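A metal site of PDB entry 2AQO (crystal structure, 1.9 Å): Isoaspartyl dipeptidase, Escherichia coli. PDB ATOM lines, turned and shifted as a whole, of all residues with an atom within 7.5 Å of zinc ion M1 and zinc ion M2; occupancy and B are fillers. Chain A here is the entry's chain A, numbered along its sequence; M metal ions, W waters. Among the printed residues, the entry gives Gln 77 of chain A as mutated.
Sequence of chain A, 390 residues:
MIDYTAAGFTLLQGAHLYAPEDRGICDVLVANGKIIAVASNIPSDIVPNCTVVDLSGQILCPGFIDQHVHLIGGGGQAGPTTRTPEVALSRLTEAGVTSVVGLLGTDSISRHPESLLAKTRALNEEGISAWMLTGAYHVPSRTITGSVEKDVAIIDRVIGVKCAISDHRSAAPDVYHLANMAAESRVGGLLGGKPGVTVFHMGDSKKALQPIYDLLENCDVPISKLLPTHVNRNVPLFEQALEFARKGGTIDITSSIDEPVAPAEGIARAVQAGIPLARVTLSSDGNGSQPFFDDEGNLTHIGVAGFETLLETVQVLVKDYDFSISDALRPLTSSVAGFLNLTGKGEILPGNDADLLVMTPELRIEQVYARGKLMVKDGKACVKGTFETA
The backbone carbonyl oxygen (O) of Leu 104 lies within hydrogen-bond range of NZ of KCX 162 (2.9 Å).
A ring nitrogen (NE2) of His 201 is in hydrogen-bond range of the guanidinium group (NH2) of Arg 169 (3.3 Å).
NE2 of His 201 lies within hydrogen-bond range of OD2 of Asp 167.
The backbone NH (N) of Gly 286 sits at hydrogen-bond distance from the backbone carbonyl oxygen (O) of His 68.
A ring nitrogen (ND1) of His 70 sits at hydrogen-bond distance from the backbone carbonyl oxygen (O) of Leu 103 (3.2 Å).
The backbone carbonyl oxygen of His 70 sits at hydrogen-bond distance from the side-chain amide nitrogen of Asn 287, at 3.2 Å.
N of Tyr 137 sits at hydrogen-bond distance from O of Gly 105.
The backbone carbonyl oxygen (O) of Tyr 137 is in hydrogen-bond range of the backbone NH (N) of Ala 164 (3.4 Å).
OH of Tyr 137 touches zinc ion M2, at 3.3 Å.
Zinc ion M1 is bound by OQ2 of KCX 162 (2.2 Å), a ring nitrogen (NE2) of His 68 (2.2 Å), the side-chain carboxylate (OD1) of Asp 285 (2.3 Å) and a ring nitrogen (NE2) of His 70 (2.3 Å).
Zinc ion M2 is bound by a ring nitrogen (NE2) of His 230 (2.2 Å), a ring nitrogen (ND1) of His 201 (2.2 Å) and OQ1 of KCX 162 (2.4 Å).
Slightly farther from zinc ion M2 lies water W1 (2.8 Å).
Water W1 bridges OH of Tyr 137 (3.0 Å) and OD2 of Asp 285 (3.5 Å).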
ATOM      1  N   HIS A  68     -28.504  20.453 -27.680  1.00  0.00           N
ATOM      2  CA  HIS A  68     -27.761  20.747 -26.470  1.00  0.00           C
ATOM      3  C   HIS A  68     -27.565  19.502 -25.652  1.00  0.00           C
ATOM      4  O   HIS A  68     -28.331  19.188 -24.745  1.00  0.00           O
ATOM      5  CB  HIS A  68     -28.537  21.762 -25.610  1.00  0.00           C
ATOM      6  CG  HIS A  68     -27.703  22.330 -24.514  1.00  0.00           C
ATOM      7  ND1 HIS A  68     -27.474  23.683 -24.436  1.00  0.00           N
ATOM      8  CD2 HIS A  68     -27.095  21.740 -23.445  1.00  0.00           C
ATOM      9  CE1 HIS A  68     -26.745  23.910 -23.357  1.00  0.00           C
ATOM     10  NE2 HIS A  68     -26.493  22.764 -22.772  1.00  0.00           N
ATOM     11  N   VAL A  69     -26.513  18.796 -26.010  1.00  0.00           N
ATOM     12  CA  VAL A  69     -26.173  17.558 -25.327  1.00  0.00           C
ATOM     13  C   VAL A  69     -24.697  17.462 -25.004  1.00  0.00           C
ATOM     14  O   VAL A  69     -23.784  17.686 -25.825  1.00  0.00           O
ATOM     15  CB  VAL A  69     -26.506  16.334 -26.213  1.00  0.00           C
ATOM     16  CG1 VAL A  69     -26.249  15.035 -25.443  1.00  0.00           C
ATOM     17  CG2 VAL A  69     -27.932  16.371 -26.765  1.00  0.00           C
ATOM     18  N   HIS A  70     -24.442  17.013 -23.778  1.00  0.00           N
ATOM     19  CA  HIS A  70     -23.079  16.769 -23.320  1.00  0.00           C
ATOM     20  C   HIS A  70     -22.606  15.364 -23.665  1.00  0.00           C
ATOM     21  O   HIS A  70     -22.427  14.498 -22.777  1.00  0.00           O
ATOM     22  CB  HIS A  70     -22.937  16.956 -21.798  1.00  0.00           C
ATOM     23  CG  HIS A  70     -23.285  18.385 -21.521  1.00  0.00           C
ATOM     24  ND1 HIS A  70     -22.357  19.406 -21.671  1.00  0.00           N
ATOM     25  CD2 HIS A  70     -24.473  18.920 -21.187  1.00  0.00           C
ATOM     26  CE1 HIS A  70     -22.984  20.519 -21.372  1.00  0.00           C
ATOM     27  NE2 HIS A  70     -24.227  20.246 -21.066  1.00  0.00           N
ATOM     28  N   GLN A  77     -18.859  19.908 -11.317  1.00  0.00           N
ATOM     29  CA  GLN A  77     -19.065  21.092 -10.491  1.00  0.00           C
ATOM     30  C   GLN A  77     -18.918  20.825  -9.015  1.00  0.00           C
ATOM     31  O   GLN A  77     -18.820  21.751  -8.256  1.00  0.00           O
ATOM     32  CB  GLN A  77     -20.472  21.740 -10.608  1.00  0.00           C
ATOM     33  CG  GLN A  77     -20.754  22.459 -11.924  1.00  0.00           C
ATOM     34  CD  GLN A  77     -21.497  21.587 -12.902  1.00  0.00           C
ATOM     35  OE1 GLN A  77     -21.941  22.226 -13.960  1.00  0.00           O
ATOM     36  NE2 GLN A  77     -21.643  20.398 -12.697  1.00  0.00           N
ATOM     37  N   LEU A 103     -21.727  19.614 -27.004  1.00  0.00           N
ATOM     38  CA  LEU A 103     -21.059  20.780 -26.449  1.00  0.00           C
ATOM     39  C   LEU A 103     -20.479  20.495 -25.074  1.00  0.00           C
ATOM     40  O   LEU A 103     -20.774  19.478 -24.450  1.00  0.00           O
ATOM     41  CB  LEU A 103     -21.985  22.051 -26.361  1.00  0.00           C
ATOM     42  CG  LEU A 103     -23.440  21.827 -25.903  1.00  0.00           C
ATOM     43  CD1 LEU A 103     -23.539  21.273 -24.489  1.00  0.00           C
ATOM     44  CD2 LEU A 103     -24.148  23.175 -25.950  1.00  0.00           C
ATOM     45  N   LEU A 104     -19.650  21.427 -24.635  1.00  0.00           N
ATOM     46  CA  LEU A 104     -18.973  21.433 -23.322  1.00  0.00           C
ATOM     47  C   LEU A 104     -19.645  22.462 -22.385  1.00  0.00           C
ATOM     48  O   LEU A 104     -20.404  23.367 -22.839  1.00  0.00           O
ATOM     49  CB  LEU A 104     -17.457  21.685 -23.444  1.00  0.00           C
ATOM     50  CG  LEU A 104     -16.705  20.699 -24.331  1.00  0.00           C
ATOM     51  CD1 LEU A 104     -15.221  21.069 -24.222  1.00  0.00           C
ATOM     52  CD2 LEU A 104     -16.936  19.258 -23.808  1.00  0.00           C
ATOM     53  N   GLY A 105     -19.392  22.336 -21.086  1.00  0.00           N
ATOM     54  CA  GLY A 105     -19.992  23.220 -20.101  1.00  0.00           C
ATOM     55  C   GLY A 105     -18.975  23.851 -19.199  1.00  0.00           C
ATOM     56  O   GLY A 105     -17.974  24.456 -19.575  1.00  0.00           O
ATOM     57  N   THR A 106     -19.282  23.711 -17.930  1.00  0.00           N
ATOM     58  CA  THR A 106     -18.465  24.306 -16.877  1.00  0.00           C
ATOM     59  C   THR A 106     -16.996  23.878 -16.964  1.00  0.00           C
ATOM     60  O   THR A 106     -16.108  24.691 -16.890  1.00  0.00           O
ATOM     61  CB  THR A 106     -19.052  23.992 -15.472  1.00  0.00           C
ATOM     62  OG1 THR A 106     -20.426  24.325 -15.469  1.00  0.00           O
ATOM     63  CG2 THR A 106     -18.403  24.854 -14.388  1.00  0.00           C
ATOM     64  N   TYR A 137     -17.892  26.985 -21.243  1.00  0.00           N
ATOM     65  CA  TYR A 137     -18.301  28.187 -20.525  1.00  0.00           C
ATOM     66  C   TYR A 137     -17.230  29.293 -20.578  1.00  0.00           C
ATOM     67  O   TYR A 137     -17.519  30.490 -20.618  1.00  0.00           O
ATOM     68  CB  TYR A 137     -18.545  27.938 -19.044  1.00  0.00           C
ATOM     69  CG  TYR A 137     -19.865  27.292 -18.622  1.00  0.00           C
ATOM     70  CD1 TYR A 137     -20.672  26.574 -19.524  1.00  0.00           C
ATOM     71  CD2 TYR A 137     -20.253  27.375 -17.281  1.00  0.00           C
ATOM     72  CE1 TYR A 137     -21.883  26.014 -19.103  1.00  0.00           C
ATOM     73  CE2 TYR A 137     -21.446  26.784 -16.841  1.00  0.00           C
ATOM     74  CZ  TYR A 137     -22.223  26.067 -17.748  1.00  0.00           C
ATOM     75  OH  TYR A 137     -23.366  25.436 -17.305  1.00  0.00           O
ATOM     76  N   KCX A 162     -19.660  27.924 -28.039  1.00  0.00           N
ATOM     77  CA  KCX A 162     -20.468  28.019 -26.840  1.00  0.00           C
ATOM     78  CB  KCX A 162     -20.520  26.595 -26.249  1.00  0.00           C
ATOM     79  CG  KCX A 162     -20.958  26.533 -24.775  1.00  0.00           C
ATOM     80  CD  KCX A 162     -22.476  26.593 -24.721  1.00  0.00           C
ATOM     81  CE  KCX A 162     -23.075  26.422 -23.317  1.00  0.00           C
ATOM     82  NZ  KCX A 162     -22.631  25.202 -22.652  1.00  0.00           N
ATOM     83  C   KCX A 162     -19.748  28.930 -25.833  1.00  0.00           C
ATOM     84  O   KCX A 162     -18.523  29.066 -25.897  1.00  0.00           O
ATOM     85  CX  KCX A 162     -23.814  24.801 -21.916  1.00  0.00           C
ATOM     86  OQ1 KCX A 162     -24.804  25.523 -21.776  1.00  0.00           O
ATOM     87  OQ2 KCX A 162     -23.658  23.640 -21.340  1.00  0.00           O
ATOM     88  N   CYS A 163     -20.488  29.489 -24.883  1.00  0.00           N
ATOM     89  CA  CYS A 163     -20.019  30.317 -23.767  1.00  0.00           C
ATOM     90  C   CYS A 163     -21.085  30.372 -22.654  1.00  0.00           C
ATOM     91  O   CYS A 163     -22.203  29.889 -22.804  1.00  0.00           O
ATOM     92  CB  CYS A 163     -19.623  31.755 -24.164  1.00  0.00           C
ATOM     93  SG  CYS A 163     -21.050  32.827 -24.563  1.00  0.00           S
ATOM     94  N   ALA A 164     -20.734  30.992 -21.529  1.00  0.00           N
ATOM     95  CA  ALA A 164     -21.659  31.178 -20.423  1.00  0.00           C
ATOM     96  C   ALA A 164     -21.643  32.637 -19.991  1.00  0.00           C
ATOM     97  O   ALA A 164     -20.578  33.267 -19.925  1.00  0.00           O
ATOM     98  CB  ALA A 164     -21.261  30.291 -19.246  1.00  0.00           C
ATOM     99  N   ASP A 167     -23.762  34.078 -14.909  1.00  0.00           N
ATOM    100  CA  ASP A 167     -23.755  32.861 -14.149  1.00  0.00           C
ATOM    101  C   ASP A 167     -22.563  32.857 -13.202  1.00  0.00           C
ATOM    102  O   ASP A 167     -21.482  33.324 -13.573  1.00  0.00           O
ATOM    103  CB  ASP A 167     -23.683  31.694 -15.148  1.00  0.00           C
ATOM    104  CG  ASP A 167     -23.804  30.350 -14.486  1.00  0.00           C
ATOM    105  OD1 ASP A 167     -22.914  29.825 -13.849  1.00  0.00           O
ATOM    106  OD2 ASP A 167     -24.964  29.814 -14.634  1.00  0.00           O
ATOM    107  N   ARG A 169     -20.696  30.628 -12.554  1.00  0.00           N
ATOM    108  CA  ARG A 169     -19.687  29.754 -13.111  1.00  0.00           C
ATOM    109  C   ARG A 169     -19.053  30.384 -14.375  1.00  0.00           C
ATOM    110  O   ARG A 169     -18.314  29.689 -15.081  1.00  0.00           O
ATOM    111  CB  ARG A 169     -20.180  28.362 -13.424  1.00  0.00           C
ATOM    112  CG  ARG A 169     -20.504  27.571 -12.168  1.00  0.00           C
ATOM    113  CD  ARG A 169     -21.528  26.466 -12.453  1.00  0.00           C
ATOM    114  NE  ARG A 169     -22.719  27.032 -13.072  1.00  0.00           N
ATOM    115  CZ  ARG A 169     -23.742  26.353 -13.592  1.00  0.00           C
ATOM    116  NH1 ARG A 169     -23.797  25.010 -13.598  1.00  0.00           N
ATOM    117  NH2 ARG A 169     -24.758  27.048 -14.119  1.00  0.00           N
ATOM    118  N   PHE A 200     -25.402  30.992 -25.801  1.00  0.00           N
ATOM    119  CA  PHE A 200     -25.118  31.465 -24.461  1.00  0.00           C
ATOM    120  C   PHE A 200     -25.841  30.727 -23.369  1.00  0.00           C
ATOM    121  O   PHE A 200     -27.054  30.838 -23.260  1.00  0.00           O
ATOM    122  CB  PHE A 200     -25.546  32.923 -24.321  1.00  0.00           C
ATOM    123  CG  PHE A 200     -24.930  33.848 -25.342  1.00  0.00           C
ATOM    124  CD1 PHE A 200     -25.420  33.885 -26.646  1.00  0.00           C
ATOM    125  CD2 PHE A 200     -23.880  34.701 -24.983  1.00  0.00           C
ATOM    126  CE1 PHE A 200     -24.850  34.732 -27.600  1.00  0.00           C
ATOM    127  CE2 PHE A 200     -23.320  35.587 -25.916  1.00  0.00           C
ATOM    128  CZ  PHE A 200     -23.805  35.579 -27.236  1.00  0.00           C
ATOM    129  N   HIS A 201     -25.077  30.005 -22.531  1.00  0.00           N
ATOM    130  CA  HIS A 201     -25.620  29.336 -21.360  1.00  0.00           C
ATOM    131  C   HIS A 201     -26.011  30.502 -20.443  1.00  0.00           C
ATOM    132  O   HIS A 201     -25.201  31.408 -20.189  1.00  0.00           O
ATOM    133  CB  HIS A 201     -24.565  28.466 -20.616  1.00  0.00           C
ATOM    134  CG  HIS A 201     -24.852  28.334 -19.147  1.00  0.00           C
ATOM    135  ND1 HIS A 201     -25.493  27.232 -18.629  1.00  0.00           N
ATOM    136  CD2 HIS A 201     -24.641  29.207 -18.123  1.00  0.00           C
ATOM    137  CE1 HIS A 201     -25.605  27.399 -17.329  1.00  0.00           C
ATOM    138  NE2 HIS A 201     -25.114  28.585 -16.992  1.00  0.00           N
ATOM    139  N   MET A 202     -27.249  30.550 -19.996  1.00  0.00           N
ATOM    140  CA  MET A 202     -27.644  31.658 -19.124  1.00  0.00           C
ATOM    141  C   MET A 202     -27.703  31.175 -17.690  1.00  0.00           C
ATOM    142  O   MET A 202     -28.220  30.077 -17.437  1.00  0.00           O
ATOM    143  CB  MET A 202     -29.073  32.169 -19.434  1.00  0.00           C
ATOM    144  CG  MET A 202     -29.234  32.711 -20.855  1.00  0.00           C
ATOM    145  SD  MET A 202     -28.037  34.002 -21.333  1.00  0.00           S
ATOM    146  CE  MET A 202     -28.295  35.303 -20.074  1.00  0.00           C
ATOM    147  N   GLY A 203     -27.230  31.970 -16.760  1.00  0.00           N
ATOM    148  CA  GLY A 203     -27.342  31.553 -15.379  1.00  0.00           C
ATOM    149  C   GLY A 203     -28.442  32.367 -14.720  1.00  0.00           C
ATOM    150  O   GLY A 203     -29.302  32.917 -15.392  1.00  0.00           O
ATOM    151  N   THR A 229     -29.866  30.054 -24.143  1.00  0.00           N
ATOM    152  CA  THR A 229     -30.433  28.773 -23.726  1.00  0.00           C
ATOM    153  C   THR A 229     -30.706  28.794 -22.215  1.00  0.00           C
ATOM    154  O   THR A 229     -30.219  29.687 -21.504  1.00  0.00           O
ATOM    155  CB  THR A 229     -29.622  27.554 -24.207  1.00  0.00           C
ATOM    156  OG1 THR A 229     -30.370  26.398 -23.910  1.00  0.00           O
ATOM    157  CG2 THR A 229     -28.281  27.474 -23.463  1.00  0.00           C
ATOM    158  N   HIS A 230     -31.524  27.833 -21.728  1.00  0.00           N
ATOM    159  CA  HIS A 230     -31.963  27.694 -20.320  1.00  0.00           C
ATOM    160  C   HIS A 230     -32.803  28.936 -19.946  1.00  0.00           C
ATOM    161  O   HIS A 230     -32.746  29.385 -18.821  1.00  0.00           O
ATOM    162  CB  HIS A 230     -30.789  27.642 -19.317  1.00  0.00           C
ATOM    163  CG  HIS A 230     -29.671  26.736 -19.730  1.00  0.00           C
ATOM    164  ND1 HIS A 230     -29.915  25.498 -20.286  1.00  0.00           N
ATOM    165  CD2 HIS A 230     -28.327  26.914 -19.637  1.00  0.00           C
ATOM    166  CE1 HIS A 230     -28.726  24.941 -20.545  1.00  0.00           C
ATOM    167  NE2 HIS A 230     -27.763  25.778 -20.166  1.00  0.00           N
ATOM    168  N   ARG A 233     -35.336  29.085 -16.788  1.00  0.00           N
ATOM    169  CA  ARG A 233     -34.701  28.904 -15.492  1.00  0.00           C
ATOM    170  C   ARG A 233     -35.124  29.852 -14.378  1.00  0.00           C
ATOM    171  O   ARG A 233     -35.038  29.514 -13.194  1.00  0.00           O
ATOM    172  CB  ARG A 233     -33.171  28.796 -15.662  1.00  0.00           C
ATOM    173  CG  ARG A 233     -32.475  30.113 -16.046  1.00  0.00           C
ATOM    174  CD  ARG A 233     -30.955  30.074 -15.988  1.00  0.00           C
ATOM    175  NE  ARG A 233     -30.492  29.319 -14.820  1.00  0.00           N
ATOM    176  CZ  ARG A 233     -29.626  28.279 -14.803  1.00  0.00           C
ATOM    177  NH1 ARG A 233     -28.999  27.779 -15.865  1.00  0.00           N
ATOM    178  NH2 ARG A 233     -29.413  27.739 -13.628  1.00  0.00           N
ATOM    179  N   THR A 254     -35.020  24.782 -22.230  1.00  0.00           N
ATOM    180  CA  THR A 254     -34.406  23.540 -21.793  1.00  0.00           C
ATOM    181  C   THR A 254     -35.449  22.623 -21.217  1.00  0.00           C
ATOM    182  O   THR A 254     -36.107  22.979 -20.225  1.00  0.00           O
ATOM    183  CB  THR A 254     -33.320  23.827 -20.751  1.00  0.00           C
ATOM    184  OG1 THR A 254     -32.350  24.675 -21.363  1.00  0.00           O
ATOM    185  CG2 THR A 254     -32.678  22.510 -20.303  1.00  0.00           C
ATOM    186  N   SER A 284     -32.393  19.455 -24.670  1.00  0.00           N
ATOM    187  CA  SER A 284     -32.420  18.775 -23.391  1.00  0.00           C
ATOM    188  C   SER A 284     -31.424  19.143 -22.301  1.00  0.00           C
ATOM    189  O   SER A 284     -31.735  19.040 -21.108  1.00  0.00           O
ATOM    190  CB  SER A 284     -32.346  17.238 -23.598  1.00  0.00           C
ATOM    191  OG  SER A 284     -31.077  16.803 -24.133  1.00  0.00           O
ATOM    192  N   ASP A 285     -30.208  19.487 -22.725  1.00  0.00           N
ATOM    193  CA  ASP A 285     -29.121  19.659 -21.801  1.00  0.00           C
ATOM    194  C   ASP A 285     -28.775  18.247 -21.249  1.00  0.00           C
ATOM    195  O   ASP A 285     -28.192  18.033 -20.165  1.00  0.00           O
ATOM    196  CB  ASP A 285     -29.338  20.727 -20.694  1.00  0.00           C
ATOM    197  CG  ASP A 285     -28.005  21.137 -20.147  1.00  0.00           C
ATOM    198  OD1 ASP A 285     -26.985  20.765 -20.677  1.00  0.00           O
ATOM    199  OD2 ASP A 285     -28.006  21.854 -19.069  1.00  0.00           O
ATOM    200  N   GLY A 286     -29.154  17.207 -22.017  1.00  0.00           N
ATOM    201  CA  GLY A 286     -28.950  15.792 -21.677  1.00  0.00           C
ATOM    202  C   GLY A 286     -27.481  15.465 -21.311  1.00  0.00           C
ATOM    203  O   GLY A 286     -26.516  16.023 -21.857  1.00  0.00           O
ATOM    204  N   ASN A 287     -27.346  14.560 -20.341  1.00  0.00           N
ATOM    205  CA  ASN A 287     -26.071  14.108 -19.880  1.00  0.00           C
ATOM    206  C   ASN A 287     -25.307  15.105 -19.013  1.00  0.00           C
ATOM    207  O   ASN A 287     -24.170  14.894 -18.605  1.00  0.00           O
ATOM    208  CB  ASN A 287     -25.217  13.499 -20.994  1.00  0.00           C
ATOM    209  CG  ASN A 287     -24.587  12.211 -20.581  1.00  0.00           C
ATOM    210  OD1 ASN A 287     -25.271  11.311 -20.081  1.00  0.00           O
ATOM    211  ND2 ASN A 287     -23.268  12.151 -20.848  1.00  0.00           N
ATOM    212  N   GLY A 288     -25.961  16.218 -18.745  1.00  0.00           N
ATOM    213  CA  GLY A 288     -25.350  17.151 -17.856  1.00  0.00           C
ATOM    214  C   GLY A 288     -25.630  16.566 -16.470  1.00  0.00           C
ATOM    215  O   GLY A 288     -26.347  15.563 -16.296  1.00  0.00           O
HETATM  216 ZN    ZN M   1     -25.331  22.285 -20.968  1.00  0.00          ZN
HETATM  217 ZN    ZN M   2     -25.734  25.272 -19.563  1.00  0.00          ZN
HETATM  218  O   HOH W   1     -24.876  22.984 -18.143  1.00  0.00           O
